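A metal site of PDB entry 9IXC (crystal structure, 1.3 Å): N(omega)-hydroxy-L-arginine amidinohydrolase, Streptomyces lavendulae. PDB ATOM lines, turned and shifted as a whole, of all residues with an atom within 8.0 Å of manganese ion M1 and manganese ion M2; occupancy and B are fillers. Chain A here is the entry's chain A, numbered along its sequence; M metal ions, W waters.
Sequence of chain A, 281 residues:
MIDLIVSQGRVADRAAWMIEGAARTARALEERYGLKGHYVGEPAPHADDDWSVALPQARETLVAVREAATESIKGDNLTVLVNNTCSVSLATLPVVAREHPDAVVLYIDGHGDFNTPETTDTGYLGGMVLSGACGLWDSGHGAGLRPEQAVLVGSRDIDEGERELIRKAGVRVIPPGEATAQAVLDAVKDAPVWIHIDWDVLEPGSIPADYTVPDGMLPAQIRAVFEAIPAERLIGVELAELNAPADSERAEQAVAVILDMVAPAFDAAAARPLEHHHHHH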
ATOM      1  N   MET A  18     -17.826  -9.501  16.638  1.00  0.00           N
ATOM      2  CA  MET A  18     -18.403  -8.252  16.153  1.00  0.00           C
ATOM      3  C   MET A  18     -19.751  -8.448  15.462  1.00  0.00           C
ATOM      4  O   MET A  18     -20.600  -7.551  15.510  1.00  0.00           O
ATOM      5  CB  MET A  18     -17.404  -7.475  15.291  1.00  0.00           C
ATOM      6  CG  MET A  18     -16.328  -6.841  16.151  1.00  0.00           C
ATOM      7  SD  MET A  18     -15.164  -5.918  15.145  1.00  0.00           S
ATOM      8  CE  MET A  18     -13.962  -5.463  16.359  1.00  0.00           C
ATOM      9  N   THR A  85     -18.458  -4.404  11.270  1.00  0.00           N
ATOM     10  CA  THR A  85     -17.139  -3.804  11.084  1.00  0.00           C
ATOM     11  C   THR A  85     -17.269  -2.462  10.378  1.00  0.00           C
ATOM     12  O   THR A  85     -18.259  -2.169   9.703  1.00  0.00           O
ATOM     13  CB  THR A  85     -16.210  -4.687  10.246  1.00  0.00           C
ATOM     14  OG1 THR A  85     -16.770  -4.871   8.934  1.00  0.00           O
ATOM     15  CG2 THR A  85     -15.953  -6.053  10.914  1.00  0.00           C
ATOM     16  N   CYS A  86     -16.237  -1.630  10.554  1.00  0.00           N
ATOM     17  CA  CYS A  86     -16.189  -0.369   9.821  1.00  0.00           C
ATOM     18  C   CYS A  86     -16.241  -0.589   8.314  1.00  0.00           C
ATOM     19  O   CYS A  86     -16.691   0.295   7.578  1.00  0.00           O
ATOM     20  CB  CYS A  86     -14.936   0.424  10.189  1.00  0.00           C
ATOM     21  SG  CYS A  86     -14.954   1.134  11.832  1.00  0.00           S
ATOM     22  N   SER A  87     -15.768  -1.739   7.836  1.00  0.00           N
ATOM     23  CA  SER A  87     -15.701  -2.009   6.401  1.00  0.00           C
ATOM     24  C   SER A  87     -17.056  -2.011   5.717  1.00  0.00           C
ATOM     25  O   SER A  87     -17.106  -1.811   4.500  1.00  0.00           O
ATOM     26  CB  SER A  87     -15.013  -3.359   6.177  1.00  0.00           C
ATOM     27  OG  SER A  87     -13.646  -3.253   6.495  1.00  0.00           O
ATOM     28  N   TYR A 107     -15.974  10.710  11.399  1.00  0.00           N
ATOM     29  CA  TYR A 107     -15.499   9.329  11.448  1.00  0.00           C
ATOM     30  C   TYR A 107     -14.807   9.176  12.807  1.00  0.00           C
ATOM     31  O   TYR A 107     -13.656   9.586  12.991  1.00  0.00           O
ATOM     32  CB  TYR A 107     -14.596   9.048  10.262  1.00  0.00           C
ATOM     33  CG  TYR A 107     -14.373   7.578   9.966  1.00  0.00           C
ATOM     34  CD1 TYR A 107     -13.454   6.840  10.699  1.00  0.00           C
ATOM     35  CD2 TYR A 107     -15.071   6.933   8.940  1.00  0.00           C
ATOM     36  CE1 TYR A 107     -13.244   5.493  10.422  1.00  0.00           C
ATOM     37  CE2 TYR A 107     -14.867   5.595   8.666  1.00  0.00           C
ATOM     38  CZ  TYR A 107     -13.950   4.870   9.389  1.00  0.00           C
ATOM     39  OH  TYR A 107     -13.744   3.524   9.103  1.00  0.00           O
ATOM     40  N   ILE A 108     -15.538   8.638  13.766  1.00  0.00           N
ATOM     41  CA  ILE A 108     -15.146   8.625  15.169  1.00  0.00           C
ATOM     42  C   ILE A 108     -14.505   7.263  15.423  1.00  0.00           C
ATOM     43  O   ILE A 108     -15.192   6.240  15.400  1.00  0.00           O
ATOM     44  CB  ILE A 108     -16.336   8.895  16.089  1.00  0.00           C
ATOM     45  CG1 ILE A 108     -17.097  10.147  15.621  1.00  0.00           C
ATOM     46  CG2 ILE A 108     -15.891   9.019  17.539  1.00  0.00           C
ATOM     47  CD1 ILE A 108     -18.264  10.520  16.503  1.00  0.00           C
ATOM     48  N   ASP A 109     -13.198   7.240  15.653  1.00  0.00           N
ATOM     49  CA  ASP A 109     -12.443   6.006  15.621  1.00  0.00           C
ATOM     50  C   ASP A 109     -11.118   6.261  16.312  1.00  0.00           C
ATOM     51  O   ASP A 109     -10.534   7.330  16.151  1.00  0.00           O
ATOM     52  CB  ASP A 109     -12.223   5.644  14.137  1.00  0.00           C
ATOM     53  CG  ASP A 109     -11.849   4.184  13.912  1.00  0.00           C
ATOM     54  OD1 ASP A 109     -11.004   3.670  14.689  1.00  0.00           O
ATOM     55  OD2 ASP A 109     -12.400   3.571  12.960  1.00  0.00           O
ATOM     56  N   GLY A 110     -10.631   5.273  17.064  1.00  0.00           N
ATOM     57  CA  GLY A 110      -9.281   5.387  17.613  1.00  0.00           C
ATOM     58  C   GLY A 110      -8.197   5.335  16.557  1.00  0.00           C
ATOM     59  O   GLY A 110      -7.068   5.770  16.813  1.00  0.00           O
ATOM     60  N   HIS A 111      -8.527   4.809  15.373  1.00  0.00           N
ATOM     61  CA  HIS A 111      -7.634   4.701  14.217  1.00  0.00           C
ATOM     62  C   HIS A 111      -8.042   5.679  13.136  1.00  0.00           C
ATOM     63  O   HIS A 111      -9.134   6.250  13.149  1.00  0.00           O
ATOM     64  CB  HIS A 111      -7.723   3.287  13.624  1.00  0.00           C
ATOM     65  CG  HIS A 111      -7.389   2.202  14.591  1.00  0.00           C
ATOM     66  ND1 HIS A 111      -8.335   1.566  15.362  1.00  0.00           N
ATOM     67  CD2 HIS A 111      -6.206   1.626  14.896  1.00  0.00           C
ATOM     68  CE1 HIS A 111      -7.745   0.650  16.118  1.00  0.00           C
ATOM     69  NE2 HIS A 111      -6.449   0.659  15.829  1.00  0.00           N
ATOM     70  N   GLY A 112      -7.145   5.853  12.146  1.00  0.00           N
ATOM     71  CA  GLY A 112      -7.482   6.655  10.980  1.00  0.00           C
ATOM     72  C   GLY A 112      -8.232   5.930   9.886  1.00  0.00           C
ATOM     73  O   GLY A 112      -8.910   6.571   9.081  1.00  0.00           O
ATOM     74  N   ASP A 113      -8.114   4.593   9.826  1.00  0.00           N
ATOM     75  CA  ASP A 113      -8.744   3.774   8.781  1.00  0.00           C
ATOM     76  C   ASP A 113      -8.482   4.364   7.381  1.00  0.00           C
ATOM     77  O   ASP A 113      -9.353   4.373   6.503  1.00  0.00           O
ATOM     78  CB  ASP A 113     -10.238   3.548   9.033  1.00  0.00           C
ATOM     79  CG  ASP A 113     -10.509   2.669  10.236  1.00  0.00           C
ATOM     80  OD1 ASP A 113      -9.557   2.268  10.933  1.00  0.00           O
ATOM     81  OD2 ASP A 113     -11.689   2.380  10.473  1.00  0.00           O
ATOM     82  N   TYR A 124      -5.466  -5.407   6.321  1.00  0.00           N
ATOM     83  CA  TYR A 124      -6.821  -5.459   6.868  1.00  0.00           C
ATOM     84  C   TYR A 124      -7.718  -4.430   6.188  1.00  0.00           C
ATOM     85  O   TYR A 124      -7.444  -3.224   6.223  1.00  0.00           O
ATOM     86  CB  TYR A 124      -6.766  -5.261   8.372  1.00  0.00           C
ATOM     87  CG  TYR A 124      -8.112  -5.291   9.033  1.00  0.00           C
ATOM     88  CD1 TYR A 124      -9.070  -6.243   8.676  1.00  0.00           C
ATOM     89  CD2 TYR A 124      -8.432  -4.371  10.014  1.00  0.00           C
ATOM     90  CE1 TYR A 124     -10.314  -6.273   9.287  1.00  0.00           C
ATOM     91  CE2 TYR A 124      -9.679  -4.379  10.628  1.00  0.00           C
ATOM     92  CZ  TYR A 124     -10.617  -5.327  10.263  1.00  0.00           C
ATOM     93  OH  TYR A 124     -11.855  -5.336  10.862  1.00  0.00           O
ATOM     94  N   LEU A 125      -8.802  -4.915   5.570  1.00  0.00           N
ATOM     95  CA  LEU A 125      -9.773  -4.047   4.914  1.00  0.00           C
ATOM     96  C   LEU A 125     -10.306  -2.978   5.863  1.00  0.00           C
ATOM     97  O   LEU A 125     -10.542  -1.836   5.449  1.00  0.00           O
ATOM     98  CB  LEU A 125     -10.924  -4.900   4.355  1.00  0.00           C
ATOM     99  CG  LEU A 125     -11.938  -4.159   3.477  1.00  0.00           C
ATOM    100  CD1 LEU A 125     -11.290  -3.682   2.184  1.00  0.00           C
ATOM    101  CD2 LEU A 125     -13.114  -5.068   3.172  1.00  0.00           C
ATOM    102  N   GLY A 126     -10.509  -3.322   7.130  1.00  0.00           N
ATOM    103  CA  GLY A 126     -11.030  -2.376   8.092  1.00  0.00           C
ATOM    104  C   GLY A 126     -10.156  -1.159   8.296  1.00  0.00           C
ATOM    105  O   GLY A 126     -10.659  -0.099   8.708  1.00  0.00           O
ATOM    106  N   GLY A 127      -8.861  -1.264   8.004  1.00  0.00           N
ATOM    107  CA  GLY A 127      -7.964  -0.132   8.079  1.00  0.00           C
ATOM    108  C   GLY A 127      -7.910   0.710   6.818  1.00  0.00           C
ATOM    109  O   GLY A 127      -7.075   1.626   6.750  1.00  0.00           O
ATOM    110  N   MET A 128      -8.768   0.429   5.842  1.00  0.00           N
ATOM    111  CA  MET A 128      -8.761   1.055   4.518  1.00  0.00           C
ATOM    112  C   MET A 128     -10.086   1.706   4.173  1.00  0.00           C
ATOM    113  O   MET A 128     -10.336   2.040   3.004  1.00  0.00           O
ATOM    114  CB  MET A 128      -8.394   0.005   3.451  1.00  0.00           C
ATOM    115  CG  MET A 128      -7.101  -0.757   3.752  1.00  0.00           C
ATOM    116  SD  MET A 128      -6.894  -2.338   2.859  1.00  0.00           S
ATOM    117  CE  MET A 128      -6.756  -1.774   1.163  1.00  0.00           C
ATOM    118  N   VAL A 129     -10.963   1.914   5.155  1.00  0.00           N
ATOM    119  CA  VAL A 129     -12.354   2.283   4.880  1.00  0.00           C
ATOM    120  C   VAL A 129     -12.481   3.745   4.454  1.00  0.00           C
ATOM    121  O   VAL A 129     -13.110   4.054   3.439  1.00  0.00           O
ATOM    122  CB  VAL A 129     -13.221   1.982   6.112  1.00  0.00           C
ATOM    123  CG1 VAL A 129     -14.641   2.478   5.895  1.00  0.00           C
ATOM    124  CG2 VAL A 129     -13.182   0.487   6.441  1.00  0.00           C
ATOM    125  N   LEU A 130     -11.919   4.653   5.250  1.00  0.00           N
ATOM    126  CA  LEU A 130     -12.143   6.067   4.967  1.00  0.00           C
ATOM    127  C   LEU A 130     -11.381   6.487   3.715  1.00  0.00           C
ATOM    128  O   LEU A 130     -11.882   7.299   2.932  1.00  0.00           O
ATOM    129  CB  LEU A 130     -11.770   6.916   6.186  1.00  0.00           C
ATOM    130  CG  LEU A 130     -12.004   8.427   6.059  1.00  0.00           C
ATOM    131  CD1 LEU A 130     -13.469   8.727   5.757  1.00  0.00           C
ATOM    132  CD2 LEU A 130     -11.554   9.111   7.340  1.00  0.00           C
ATOM    133  N   LEU A 152     -11.759  12.990  11.120  1.00  0.00           N
ATOM    134  CA  LEU A 152     -11.460  11.945  12.080  1.00  0.00           C
ATOM    135  C   LEU A 152     -11.580  12.514  13.490  1.00  0.00           C
ATOM    136  O   LEU A 152     -10.996  13.571  13.789  1.00  0.00           O
ATOM    137  CB  LEU A 152     -10.054  11.406  11.820  1.00  0.00           C
ATOM    138  CG  LEU A 152      -9.967  10.447  10.626  1.00  0.00           C
ATOM    139  CD1 LEU A 152      -8.529  10.262  10.181  1.00  0.00           C
ATOM    140  CD2 LEU A 152     -10.591   9.089  10.987  1.00  0.00           C
ATOM    141  N   SER A 155      -9.105   9.949  16.909  1.00  0.00           N
ATOM    142  CA  SER A 155      -7.990   9.156  16.421  1.00  0.00           C
ATOM    143  C   SER A 155      -6.695   9.601  17.085  1.00  0.00           C
ATOM    144  O   SER A 155      -6.494  10.787  17.395  1.00  0.00           O
ATOM    145  CB  SER A 155      -7.884   9.315  14.908  1.00  0.00           C
ATOM    146  OG  SER A 155      -9.151   9.153  14.294  1.00  0.00           O
ATOM    147  N   HIS A 196     -20.156   8.196  11.947  1.00  0.00           N
ATOM    148  CA  HIS A 196     -19.680   6.813  11.921  1.00  0.00           C
ATOM    149  C   HIS A 196     -18.843   6.582  13.170  1.00  0.00           C
ATOM    150  O   HIS A 196     -17.880   7.310  13.401  1.00  0.00           O
ATOM    151  CB  HIS A 196     -18.813   6.628  10.666  1.00  0.00           C
ATOM    152  CG  HIS A 196     -18.068   5.317  10.615  1.00  0.00           C
ATOM    153  ND1 HIS A 196     -18.410   4.314   9.733  1.00  0.00           N
ATOM    154  CD2 HIS A 196     -17.008   4.866  11.312  1.00  0.00           C
ATOM    155  CE1 HIS A 196     -17.583   3.283   9.915  1.00  0.00           C
ATOM    156  NE2 HIS A 196     -16.735   3.600  10.874  1.00  0.00           N
ATOM    157  N   ILE A 197     -19.193   5.584  13.993  1.00  0.00           N
ATOM    158  CA  ILE A 197     -18.439   5.313  15.219  1.00  0.00           C
ATOM    159  C   ILE A 197     -17.889   3.900  15.217  1.00  0.00           C
ATOM    160  O   ILE A 197     -18.634   2.930  15.003  1.00  0.00           O
ATOM    161  CB  ILE A 197     -19.282   5.524  16.487  1.00  0.00           C
ATOM    162  CG1 ILE A 197     -19.885   6.916  16.519  1.00  0.00           C
ATOM    163  CG2 ILE A 197     -18.410   5.281  17.732  1.00  0.00           C
ATOM    164  CD1 ILE A 197     -20.863   7.070  17.655  1.00  0.00           C
ATOM    165  N   ASP A 198     -16.584   3.778  15.477  1.00  0.00           N
ATOM    166  CA  ASP A 198     -15.915   2.528  15.842  1.00  0.00           C
ATOM    167  C   ASP A 198     -15.668   2.601  17.334  1.00  0.00           C
ATOM    168  O   ASP A 198     -14.972   3.505  17.821  1.00  0.00           O
ATOM    169  CB  ASP A 198     -14.589   2.501  15.069  1.00  0.00           C
ATOM    170  CG  ASP A 198     -13.677   1.319  15.407  1.00  0.00           C
ATOM    171  OD1 ASP A 198     -13.846   0.666  16.438  1.00  0.00           O
ATOM    172  OD2 ASP A 198     -12.749   1.108  14.599  1.00  0.00           O
ATOM    173  N   TRP A 199     -16.224   1.643  18.086  1.00  0.00           N
ATOM    174  CA  TRP A 199     -16.132   1.714  19.552  1.00  0.00           C
ATOM    175  C   TRP A 199     -14.715   1.647  20.102  1.00  0.00           C
ATOM    176  O   TRP A 199     -14.520   1.991  21.279  1.00  0.00           O
ATOM    177  CB  TRP A 199     -17.033   0.670  20.230  1.00  0.00           C
ATOM    178  CG  TRP A 199     -18.476   0.859  19.885  1.00  0.00           C
ATOM    179  CD1 TRP A 199     -19.266  -0.037  19.230  1.00  0.00           C
ATOM    180  CD2 TRP A 199     -19.286   2.019  20.118  1.00  0.00           C
ATOM    181  NE1 TRP A 199     -20.527   0.481  19.060  1.00  0.00           N
ATOM    182  CE2 TRP A 199     -20.573   1.741  19.594  1.00  0.00           C
ATOM    183  CE3 TRP A 199     -19.069   3.253  20.732  1.00  0.00           C
ATOM    184  CZ2 TRP A 199     -21.621   2.657  19.654  1.00  0.00           C
ATOM    185  CZ3 TRP A 199     -20.106   4.153  20.787  1.00  0.00           C
ATOM    186  CH2 TRP A 199     -21.376   3.851  20.256  1.00  0.00           C
ATOM    187  N   ASP A 200     -13.705   1.262  19.312  1.00  0.00           N
ATOM    188  CA  ASP A 200     -12.343   1.316  19.834  1.00  0.00           C
ATOM    189  C   ASP A 200     -11.858   2.741  20.062  1.00  0.00           C
ATOM    190  O   ASP A 200     -10.768   2.931  20.584  1.00  0.00           O
ATOM    191  CB  ASP A 200     -11.347   0.475  19.014  1.00  0.00           C
ATOM    192  CG  ASP A 200     -11.066   1.005  17.605  1.00  0.00           C
ATOM    193  OD1 ASP A 200     -11.216   2.217  17.331  1.00  0.00           O
ATOM    194  OD2 ASP A 200     -10.697   0.153  16.768  1.00  0.00           O
ATOM    195  N   VAL A 201     -12.659   3.744  19.699  1.00  0.00           N
ATOM    196  CA  VAL A 201     -12.358   5.119  20.081  1.00  0.00           C
ATOM    197  C   VAL A 201     -12.398   5.308  21.600  1.00  0.00           C
ATOM    198  O   VAL A 201     -11.734   6.217  22.121  1.00  0.00           O
ATOM    199  CB  VAL A 201     -13.276   6.121  19.356  1.00  0.00           C
ATOM    200  CG1 VAL A 201     -14.690   6.099  19.957  1.00  0.00           C
ATOM    201  CG2 VAL A 201     -12.662   7.532  19.385  1.00  0.00           C
ATOM    202  N   ALA A 240     -20.387   0.696  14.892  1.00  0.00           N
ATOM    203  CA  ALA A 240     -19.589  -0.418  14.430  1.00  0.00           C
ATOM    204  C   ALA A 240     -18.579  -0.904  15.467  1.00  0.00           C
ATOM    205  O   ALA A 240     -18.095  -0.143  16.310  1.00  0.00           O
ATOM    206  CB  ALA A 240     -18.828  -0.047  13.134  1.00  0.00           C
ATOM    207  N   GLU A 241     -18.288  -2.200  15.385  1.00  0.00           N
ATOM    208  CA  GLU A 241     -17.128  -2.836  16.050  1.00  0.00           C
ATOM    209  C   GLU A 241     -17.302  -2.957  17.569  1.00  0.00           C
ATOM    210  O   GLU A 241     -16.414  -2.585  18.354  1.00  0.00           O
ATOM    211  CB  GLU A 241     -15.804  -2.184  15.661  1.00  0.00           C
ATOM    212  CG  GLU A 241     -15.668  -2.029  14.147  1.00  0.00           C
ATOM    213  CD  GLU A 241     -14.324  -2.419  13.572  1.00  0.00           C
ATOM    214  OE1 GLU A 241     -13.370  -2.690  14.346  1.00  0.00           O
ATOM    215  OE2 GLU A 241     -14.212  -2.412  12.331  1.00  0.00           O
HETATM  216 MN    MN M   1     -12.539   1.507  12.357  1.00  0.00          MN
HETATM  217 MN    MN M   2     -10.594   1.622  15.131  1.00  0.00          MN
HETATM  218  O   HOH W   1     -12.202  -0.571  11.702  1.00  0.00           O
HETATM  219  O   HOH W   2     -10.374   1.024  12.997  1.00  0.00           O
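Water W1 lies within hydrogen-bond range of the side-chain carboxylate (OE2) of Glu 241 and the backbone carbonyl oxygen (O) of Gly 126.
The side-chain carboxylate (OD1) of Asp 109 is bound to manganese ion M2 (2.1 Å). Manganese ion M2 is bound by OD2 of Asp 200 (2.2 Å). Water W2 is bound to manganese ion M2 (2.2 Å). ND1 of His 111 binds manganese ion M2, 2.3 Å away. Manganese ion M2 is bound by the side-chain carboxylate (OD2) of Asp 198 (2.3 Å). OD1 of Asp 200 binds manganese ion M2 (2.4 Å). Manganese ion M2 has six donor atoms within binding distance.
Manganese ion M1 is bound by OD2 of Asp 109 (2.2 Å), water W1 (2.2 Å), OD2 of Asp 113 (2.2 Å), OD2 of Asp 198 (2.3 Å), water W2 (2.3 Å) and SG of Cys 86 (2.5 Å).
The backbone carbonyl oxygen (O) of His 111 lies within hydrogen-bond range of the side-chain hydroxyl (OG) of Ser 155 (3.1 Å). OD1 of Asp 200 lies close to N of Gly 110 (3.1 Å). The side-chain hydroxyl (OG) of Ser 155 is in hydrogen-bond range of the backbone carbonyl oxygen (O) of Asp 109, 2.9 Å away. OD2 of Asp 113 lies close to OH of Tyr 107 (2.7 Å). O of Asp 113 lies within hydrogen-bond range of N of Val 129, at 3.2 Å. A ring nitrogen (NE2) of His 196 sits close to the side-chain sulfur (SG) of Cys 86 (3.2 Å). N of Cys 86 sits at hydrogen-bond distance from OE2 of Glu 241, at 2.8 Å. The backbone NH (N) of Asp 198 lies within hydrogen-bond range of the backbone carbonyl oxygen (O) of Ile 108 (2.8 Å).
Within 4 Å of manganese ion M2: Asp 109, His 111, Asp 198 and Asp 200.
Four residues have an atom within 4 Å of manganese ion M1: Cys 86, Asp 109, Asp 113 and Asp 198.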
